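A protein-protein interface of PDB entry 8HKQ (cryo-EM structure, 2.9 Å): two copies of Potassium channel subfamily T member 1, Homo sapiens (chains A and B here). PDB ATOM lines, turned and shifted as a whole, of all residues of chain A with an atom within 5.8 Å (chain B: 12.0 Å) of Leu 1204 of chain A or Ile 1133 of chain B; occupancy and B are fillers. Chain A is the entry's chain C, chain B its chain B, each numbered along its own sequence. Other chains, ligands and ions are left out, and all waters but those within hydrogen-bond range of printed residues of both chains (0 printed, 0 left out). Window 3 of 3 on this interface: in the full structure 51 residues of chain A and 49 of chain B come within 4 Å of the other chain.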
ATOM      1  N   LYS A 751      14.648 -32.473  16.534  1.00  0.00           N
ATOM      2  CA  LYS A 751      13.497 -31.581  16.624  1.00  0.00           C
ATOM      3  C   LYS A 751      12.960 -31.350  15.219  1.00  0.00           C
ATOM      4  O   LYS A 751      13.668 -30.814  14.360  1.00  0.00           O
ATOM      5  CB  LYS A 751      13.875 -30.263  17.297  1.00  0.00           C
ATOM      6  CG  LYS A 751      13.970 -30.354  18.811  1.00  0.00           C
ATOM      7  CD  LYS A 751      14.388 -29.031  19.424  1.00  0.00           C
ATOM      8  CE  LYS A 751      14.509 -29.143  20.934  1.00  0.00           C
ATOM      9  NZ  LYS A 751      14.997 -27.878  21.547  1.00  0.00           N
ATOM     10  N   GLY A 752      11.719 -31.756  14.989  1.00  0.00           N
ATOM     11  CA  GLY A 752      11.109 -31.584  13.685  1.00  0.00           C
ATOM     12  C   GLY A 752       9.639 -31.927  13.744  1.00  0.00           C
ATOM     13  O   GLY A 752       9.112 -32.336  14.781  1.00  0.00           O
ATOM     14  N   TYR A 753       8.994 -31.751  12.629  1.00  0.00           N
ATOM     15  CA  TYR A 753       7.576 -32.060  12.573  1.00  0.00           C
ATOM     16  C   TYR A 753       7.361 -33.551  12.336  1.00  0.00           C
ATOM     17  O   TYR A 753       8.180 -34.205  11.682  1.00  0.00           O
ATOM     18  CB  TYR A 753       6.904 -31.261  11.462  1.00  0.00           C
ATOM     19  CG  TYR A 753       6.951 -29.770  11.692  1.00  0.00           C
ATOM     20  CD1 TYR A 753       8.048 -29.021  11.290  1.00  0.00           C
ATOM     21  CD2 TYR A 753       5.908 -29.114  12.325  1.00  0.00           C
ATOM     22  CE1 TYR A 753       8.098 -27.659  11.504  1.00  0.00           C
ATOM     23  CE2 TYR A 753       5.949 -27.754  12.543  1.00  0.00           C
ATOM     24  CZ  TYR A 753       7.044 -27.032  12.131  1.00  0.00           C
ATOM     25  OH  TYR A 753       7.084 -25.676  12.350  1.00  0.00           O
ATOM     26  N   LEU A 766       6.216 -28.476  15.917  1.00  0.00           N
ATOM     27  CA  LEU A 766       7.587 -28.923  16.119  1.00  0.00           C
ATOM     28  C   LEU A 766       7.659 -29.758  17.391  1.00  0.00           C
ATOM     29  O   LEU A 766       7.320 -29.277  18.477  1.00  0.00           O
ATOM     30  CB  LEU A 766       8.528 -27.724  16.204  1.00  0.00           C
ATOM     31  CG  LEU A 766       9.988 -27.969  15.817  1.00  0.00           C
ATOM     32  CD1 LEU A 766      10.170 -27.875  14.314  1.00  0.00           C
ATOM     33  CD2 LEU A 766      10.904 -26.991  16.533  1.00  0.00           C
ATOM     34  N   TYR A 824       8.285 -29.322  21.192  1.00  0.00           N
ATOM     35  CA  TYR A 824       9.689 -28.945  21.305  1.00  0.00           C
ATOM     36  C   TYR A 824       9.967 -28.050  22.507  1.00  0.00           C
ATOM     37  O   TYR A 824      11.089 -28.070  23.025  1.00  0.00           O
ATOM     38  CB  TYR A 824      10.159 -28.256  20.023  1.00  0.00           C
ATOM     39  CG  TYR A 824       9.702 -26.821  19.872  1.00  0.00           C
ATOM     40  CD1 TYR A 824       8.395 -26.520  19.517  1.00  0.00           C
ATOM     41  CD2 TYR A 824      10.585 -25.768  20.071  1.00  0.00           C
ATOM     42  CE1 TYR A 824       7.976 -25.213  19.371  1.00  0.00           C
ATOM     43  CE2 TYR A 824      10.174 -24.456  19.930  1.00  0.00           C
ATOM     44  CZ  TYR A 824       8.870 -24.184  19.580  1.00  0.00           C
ATOM     45  OH  TYR A 824       8.454 -22.881  19.438  1.00  0.00           O
ATOM     46  N   ASP A1202       6.706 -17.196  22.669  1.00  0.00           N
ATOM     47  CA  ASP A1202       7.244 -18.147  21.705  1.00  0.00           C
ATOM     48  C   ASP A1202       8.768 -18.121  21.733  1.00  0.00           C
ATOM     49  O   ASP A1202       9.368 -17.051  21.570  1.00  0.00           O
ATOM     50  CB  ASP A1202       6.728 -17.813  20.308  1.00  0.00           C
ATOM     51  CG  ASP A1202       7.039 -18.892  19.297  1.00  0.00           C
ATOM     52  OD1 ASP A1202       6.308 -19.903  19.260  1.00  0.00           O
ATOM     53  OD2 ASP A1202       8.005 -18.722  18.529  1.00  0.00           O
ATOM     54  N   PRO A1203       9.429 -19.263  21.933  1.00  0.00           N
ATOM     55  CA  PRO A1203      10.897 -19.272  21.967  1.00  0.00           C
ATOM     56  C   PRO A1203      11.504 -19.095  20.586  1.00  0.00           C
ATOM     57  O   PRO A1203      12.673 -18.720  20.453  1.00  0.00           O
ATOM     58  CB  PRO A1203      11.232 -20.654  22.551  1.00  0.00           C
ATOM     59  CG  PRO A1203       9.918 -21.229  23.031  1.00  0.00           C
ATOM     60  CD  PRO A1203       8.870 -20.600  22.178  1.00  0.00           C
ATOM     61  N   LEU A1204      10.712 -19.366  19.550  1.00  0.00           N
ATOM     62  CA  LEU A1204      11.204 -19.352  18.179  1.00  0.00           C
ATOM     63  C   LEU A1204      11.138 -17.976  17.532  1.00  0.00           C
ATOM     64  O   LEU A1204      11.922 -17.700  16.617  1.00  0.00           O
ATOM     65  CB  LEU A1204      10.402 -20.344  17.332  1.00  0.00           C
ATOM     66  CG  LEU A1204      10.814 -21.814  17.393  1.00  0.00           C
ATOM     67  CD1 LEU A1204      10.417 -22.531  16.114  1.00  0.00           C
ATOM     68  CD2 LEU A1204      12.305 -21.957  17.659  1.00  0.00           C
ATOM     69  N   ALA A1205      10.231 -17.115  17.981  1.00  0.00           N
ATOM     70  CA  ALA A1205      10.072 -15.791  17.392  1.00  0.00           C
ATOM     71  C   ALA A1205      11.018 -14.785  18.038  1.00  0.00           C
ATOM     72  O   ALA A1205      11.963 -15.163  18.730  1.00  0.00           O
ATOM     73  CB  ALA A1205       8.631 -15.323  17.525  1.00  0.00           C
ATOM     74  N   ALA B1129      20.450 -23.630  13.815  1.00  0.00           N
ATOM     75  CA  ALA B1129      19.413 -24.278  13.022  1.00  0.00           C
ATOM     76  C   ALA B1129      18.058 -23.620  13.250  1.00  0.00           C
ATOM     77  O   ALA B1129      17.060 -24.012  12.645  1.00  0.00           O
ATOM     78  CB  ALA B1129      19.342 -25.762  13.347  1.00  0.00           C
ATOM     79  N   ALA B1130      18.034 -22.610  14.124  1.00  0.00           N
ATOM     80  CA  ALA B1130      16.780 -21.939  14.454  1.00  0.00           C
ATOM     81  C   ALA B1130      16.169 -21.269  13.230  1.00  0.00           C
ATOM     82  O   ALA B1130      14.948 -21.305  13.036  1.00  0.00           O
ATOM     83  CB  ALA B1130      17.008 -20.918  15.568  1.00  0.00           C
ATOM     84  N   GLU B1131      17.002 -20.649  12.392  1.00  0.00           N
ATOM     85  CA  GLU B1131      16.486 -19.986  11.200  1.00  0.00           C
ATOM     86  C   GLU B1131      15.820 -20.981  10.256  1.00  0.00           C
ATOM     87  O   GLU B1131      14.760 -20.693   9.687  1.00  0.00           O
ATOM     88  CB  GLU B1131      17.613 -19.238  10.490  1.00  0.00           C
ATOM     89  CG  GLU B1131      18.152 -18.050  11.272  1.00  0.00           C
ATOM     90  CD  GLU B1131      19.337 -17.394  10.593  1.00  0.00           C
ATOM     91  OE1 GLU B1131      19.855 -17.969   9.613  1.00  0.00           O
ATOM     92  OE2 GLU B1131      19.751 -16.301  11.037  1.00  0.00           O
ATOM     93  N   TRP B1132      16.419 -22.163  10.088  1.00  0.00           N
ATOM     94  CA  TRP B1132      15.870 -23.151   9.163  1.00  0.00           C
ATOM     95  C   TRP B1132      14.503 -23.651   9.618  1.00  0.00           C
ATOM     96  O   TRP B1132      13.553 -23.701   8.822  1.00  0.00           O
ATOM     97  CB  TRP B1132      16.842 -24.322   9.015  1.00  0.00           C
ATOM     98  CG  TRP B1132      18.125 -23.959   8.332  1.00  0.00           C
ATOM     99  CD1 TRP B1132      19.283 -23.547   8.927  1.00  0.00           C
ATOM    100  CD2 TRP B1132      18.382 -23.975   6.923  1.00  0.00           C
ATOM    101  NE1 TRP B1132      20.244 -23.306   7.975  1.00  0.00           N
ATOM    102  CE2 TRP B1132      19.716 -23.562   6.737  1.00  0.00           C
ATOM    103  CE3 TRP B1132      17.613 -24.299   5.801  1.00  0.00           C
ATOM    104  CZ2 TRP B1132      20.297 -23.463   5.475  1.00  0.00           C
ATOM    105  CZ3 TRP B1132      18.192 -24.201   4.550  1.00  0.00           C
ATOM    106  CH2 TRP B1132      19.520 -23.787   4.397  1.00  0.00           C
ATOM    107  N   ILE B1133      14.378 -24.027  10.892  1.00  0.00           N
ATOM    108  CA  ILE B1133      13.091 -24.518  11.367  1.00  0.00           C
ATOM    109  C   ILE B1133      12.072 -23.391  11.482  1.00  0.00           C
ATOM    110  O   ILE B1133      10.873 -23.648  11.362  1.00  0.00           O
ATOM    111  CB  ILE B1133      13.231 -25.285  12.695  1.00  0.00           C
ATOM    112  CG1 ILE B1133      14.140 -24.555  13.683  1.00  0.00           C
ATOM    113  CG2 ILE B1133      13.755 -26.693  12.446  1.00  0.00           C
ATOM    114  CD1 ILE B1133      13.431 -23.542  14.541  1.00  0.00           C
ATOM    115  N   SER B1134      12.510 -22.144  11.673  1.00  0.00           N
ATOM    116  CA  SER B1134      11.575 -21.025  11.588  1.00  0.00           C
ATOM    117  C   SER B1134      11.036 -20.863  10.170  1.00  0.00           C
ATOM    118  O   SER B1134       9.837 -20.619   9.976  1.00  0.00           O
ATOM    119  CB  SER B1134      12.252 -19.738  12.053  1.00  0.00           C
ATOM    120  OG  SER B1134      13.301 -19.373  11.175  1.00  0.00           O
ATOM    121  N   GLN B1135      11.912 -20.980   9.168  1.00  0.00           N
ATOM    122  CA  GLN B1135      11.487 -20.960   7.774  1.00  0.00           C
ATOM    123  C   GLN B1135      10.455 -22.048   7.509  1.00  0.00           C
ATOM    124  O   GLN B1135       9.405 -21.801   6.904  1.00  0.00           O
ATOM    125  CB  GLN B1135      12.696 -21.141   6.849  1.00  0.00           C
ATOM    126  CG  GLN B1135      13.682 -19.987   6.843  1.00  0.00           C
ATOM    127  CD  GLN B1135      14.955 -20.319   6.087  1.00  0.00           C
ATOM    128  OE1 GLN B1135      15.332 -21.485   5.964  1.00  0.00           O
ATOM    129  NE2 GLN B1135      15.624 -19.293   5.574  1.00  0.00           N
ATOM    130  N   GLN B1136      10.754 -23.267   7.965  1.00  0.00           N
ATOM    131  CA  GLN B1136       9.811 -24.370   7.801  1.00  0.00           C
ATOM    132  C   GLN B1136       8.504 -24.105   8.541  1.00  0.00           C
ATOM    133  O   GLN B1136       7.431 -24.480   8.055  1.00  0.00           O
ATOM    134  CB  GLN B1136      10.444 -25.677   8.275  1.00  0.00           C
ATOM    135  CG  GLN B1136      11.608 -26.158   7.423  1.00  0.00           C
ATOM    136  CD  GLN B1136      12.252 -27.416   7.968  1.00  0.00           C
ATOM    137  OE1 GLN B1136      12.177 -27.698   9.165  1.00  0.00           O
ATOM    138  NE2 GLN B1136      12.887 -28.184   7.091  1.00  0.00           N
ATOM    139  N   ARG B1137       8.573 -23.458   9.706  1.00  0.00           N
ATOM    140  CA  ARG B1137       7.373 -23.130  10.467  1.00  0.00           C
ATOM    141  C   ARG B1137       6.465 -22.191   9.687  1.00  0.00           C
ATOM    142  O   ARG B1137       5.259 -22.440   9.558  1.00  0.00           O
ATOM    143  CB  ARG B1137       7.772 -22.507  11.806  1.00  0.00           C
ATOM    144  CG  ARG B1137       6.629 -21.877  12.581  1.00  0.00           C
ATOM    145  CD  ARG B1137       7.155 -21.164  13.815  1.00  0.00           C
ATOM    146  NE  ARG B1137       7.054 -21.993  15.009  1.00  0.00           N
ATOM    147  CZ  ARG B1137       6.996 -21.520  16.246  1.00  0.00           C
ATOM    148  NH1 ARG B1137       7.026 -20.221  16.491  1.00  0.00           N
ATOM    149  NH2 ARG B1137       6.905 -22.372  17.264  1.00  0.00           N
ATOM    150  N   LEU B1138       7.027 -21.102   9.156  1.00  0.00           N
ATOM    151  CA  LEU B1138       6.211 -20.198   8.348  1.00  0.00           C
ATOM    152  C   LEU B1138       5.714 -20.871   7.074  1.00  0.00           C
ATOM    153  O   LEU B1138       4.584 -20.614   6.643  1.00  0.00           O
ATOM    154  CB  LEU B1138       6.970 -18.915   8.003  1.00  0.00           C
ATOM    155  CG  LEU B1138       7.162 -17.874   9.110  1.00  0.00           C
ATOM    156  CD1 LEU B1138       8.574 -17.874   9.661  1.00  0.00           C
ATOM    157  CD2 LEU B1138       6.774 -16.487   8.612  1.00  0.00           C
ATOM    158  N   SER B1139       6.532 -21.730   6.459  1.00  0.00           N
ATOM    159  CA  SER B1139       6.101 -22.422   5.249  1.00  0.00           C
ATOM    160  C   SER B1139       4.901 -23.322   5.525  1.00  0.00           C
ATOM    161  O   SER B1139       3.939 -23.348   4.750  1.00  0.00           O
ATOM    162  CB  SER B1139       7.262 -23.230   4.669  1.00  0.00           C
ATOM    163  OG  SER B1139       8.307 -22.377   4.236  1.00  0.00           O
ATOM    164  N   LEU B1140       4.943 -24.070   6.630  1.00  0.00           N
ATOM    165  CA  LEU B1140       3.819 -24.934   6.977  1.00  0.00           C
ATOM    166  C   LEU B1140       2.602 -24.131   7.413  1.00  0.00           C
ATOM    167  O   LEU B1140       1.466 -24.543   7.152  1.00  0.00           O
ATOM    168  CB  LEU B1140       4.226 -25.919   8.072  1.00  0.00           C
ATOM    169  CG  LEU B1140       5.065 -27.112   7.612  1.00  0.00           C
ATOM    170  CD1 LEU B1140       5.927 -27.627   8.748  1.00  0.00           C
ATOM    171  CD2 LEU B1140       4.177 -28.218   7.067  1.00  0.00           C
ATOM    172  N   TYR B1141       2.810 -22.990   8.077  1.00  0.00           N
ATOM    173  CA  TYR B1141       1.680 -22.155   8.468  1.00  0.00           C
ATOM    174  C   TYR B1141       0.996 -21.531   7.259  1.00  0.00           C
ATOM    175  O   TYR B1141      -0.229 -21.365   7.258  1.00  0.00           O
ATOM    176  CB  TYR B1141       2.140 -21.068   9.439  1.00  0.00           C
ATOM    177  CG  TYR B1141       1.034 -20.136   9.883  1.00  0.00           C
ATOM    178  CD1 TYR B1141      -0.029 -20.601  10.646  1.00  0.00           C
ATOM    179  CD2 TYR B1141       1.056 -18.791   9.541  1.00  0.00           C
ATOM    180  CE1 TYR B1141      -1.040 -19.752  11.054  1.00  0.00           C
ATOM    181  CE2 TYR B1141       0.050 -17.935   9.944  1.00  0.00           C
ATOM    182  CZ  TYR B1141      -0.995 -18.421  10.700  1.00  0.00           C
ATOM    183  OH  TYR B1141      -2.001 -17.573  11.104  1.00  0.00           O
ATOM    184  N   ARG B1142       1.762 -21.178   6.230  1.00  0.00           N
ATOM    185  CA  ARG B1142       1.212 -20.566   5.028  1.00  0.00           C
ATOM    186  C   ARG B1142       0.699 -21.581   4.014  1.00  0.00           C
ATOM    187  O   ARG B1142       0.060 -21.183   3.034  1.00  0.00           O
ATOM    188  CB  ARG B1142       2.266 -19.674   4.364  1.00  0.00           C
ATOM    189  CG  ARG B1142       2.632 -18.438   5.170  1.00  0.00           C
ATOM    190  CD  ARG B1142       3.044 -17.292   4.262  1.00  0.00           C
ATOM    191  NE  ARG B1142       1.915 -16.441   3.907  1.00  0.00           N
ATOM    192  CZ  ARG B1142       2.010 -15.149   3.624  1.00  0.00           C
ATOM    193  NH1 ARG B1142       3.174 -14.521   3.643  1.00  0.00           N
ATOM    194  NH2 ARG B1142       0.910 -14.471   3.313  1.00  0.00           N
ATOM    195  N   ARG B1143       0.959 -22.870   4.218  1.00  0.00           N
ATOM    196  CA  ARG B1143       0.507 -23.879   3.270  1.00  0.00           C
ATOM    197  C   ARG B1143      -1.002 -24.068   3.369  1.00  0.00           C
ATOM    198  O   ARG B1143      -1.590 -23.966   4.449  1.00  0.00           O
ATOM    199  CB  ARG B1143       1.248 -25.198   3.505  1.00  0.00           C
ATOM    200  CG  ARG B1143       0.451 -26.301   4.179  1.00  0.00           C
ATOM    201  CD  ARG B1143       1.330 -27.526   4.386  1.00  0.00           C
ATOM    202  NE  ARG B1143       0.656 -28.595   5.113  1.00  0.00           N
ATOM    203  CZ  ARG B1143       0.474 -28.609   6.426  1.00  0.00           C
ATOM    204  NH1 ARG B1143       0.888 -27.615   7.193  1.00  0.00           N
ATOM    205  NH2 ARG B1143      -0.138 -29.649   6.985  1.00  0.00           N
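Printed residues of chain A that touch a printed residue of chain B: Tyr 753, Tyr 824, Asp 1202 and Leu 1204. Hydrophobic or aromatic side chains of chain A within 4 Å of the printed part of chain B: Tyr 753, Tyr 824 and Leu 1204.
Of chain B, only Ile 1133 and Arg 1137 come within 4 Å of Leu 1204 of chain A. Printed residues of chain A within 4 Å of Ile 1133 of chain B: Leu 1204. No residue of chain B comes within 4 Å of Gly 752 of chain A. No residue of chain B comes within 4 Å of Leu 766 of chain A. Printed residues of chain B within 4 Å of Tyr 753 of chain A: Arg 1137 and Leu 1140. Printed residues of chain B within 4 Å of Tyr 824 of chain A: Arg 1137 (2.7 Å). The nearest residue of chain B that does not touch Leu 1204 of chain A is Ser 1134 of chain B (4.9 Å). The nearest printed residue of chain A that does not touch Leu 1140 of chain B is Leu 766 of chain A (7.0 Å).
OD2 of Asp 1202 of chain A is in hydrogen-bond range of N of Leu 1204 of chain A (3.0 Å). O of Leu 1140 of chain B lies within hydrogen-bond range of NH1 of Arg 1143 of chain B (3.1 Å). N of Ala 1205 of chain A is in hydrogen-bond range of OD2 of Asp 1202 of chain A (2.8 Å). The backbone carbonyl oxygen (O) of Leu 766 of chain A lies within hydrogen-bond range of the backbone NH (N) of Tyr 824 of chain A, at 2.9 Å.
Among the printed residues, merely in contact across the chains: Tyr 753 of chain A with Arg 1137 of chain B, Tyr 753 of chain A with Leu 1140 of chain B, Leu 1204 of chain A with Ile 1133 of chain B and Leu 1204 of chain A with Arg 1137 of chain B.
The side-chain carboxylate (OD2) of Asp 1202 of chain A is in salt-bridge range of the guanidinium group (NH1) of Arg 1137 of chain B, at 2.7 Å. The side-chain hydroxyl (OH) of Tyr 824 of chain A lies within hydrogen-bond range of the guanidinium group (NH2) of Arg 1137 of chain B, 2.7 Å away.
No position is printed for both chains. Of the 6 pairs that touch across the chains among the printed residues, none has its exchanged pair printed and touching as well.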
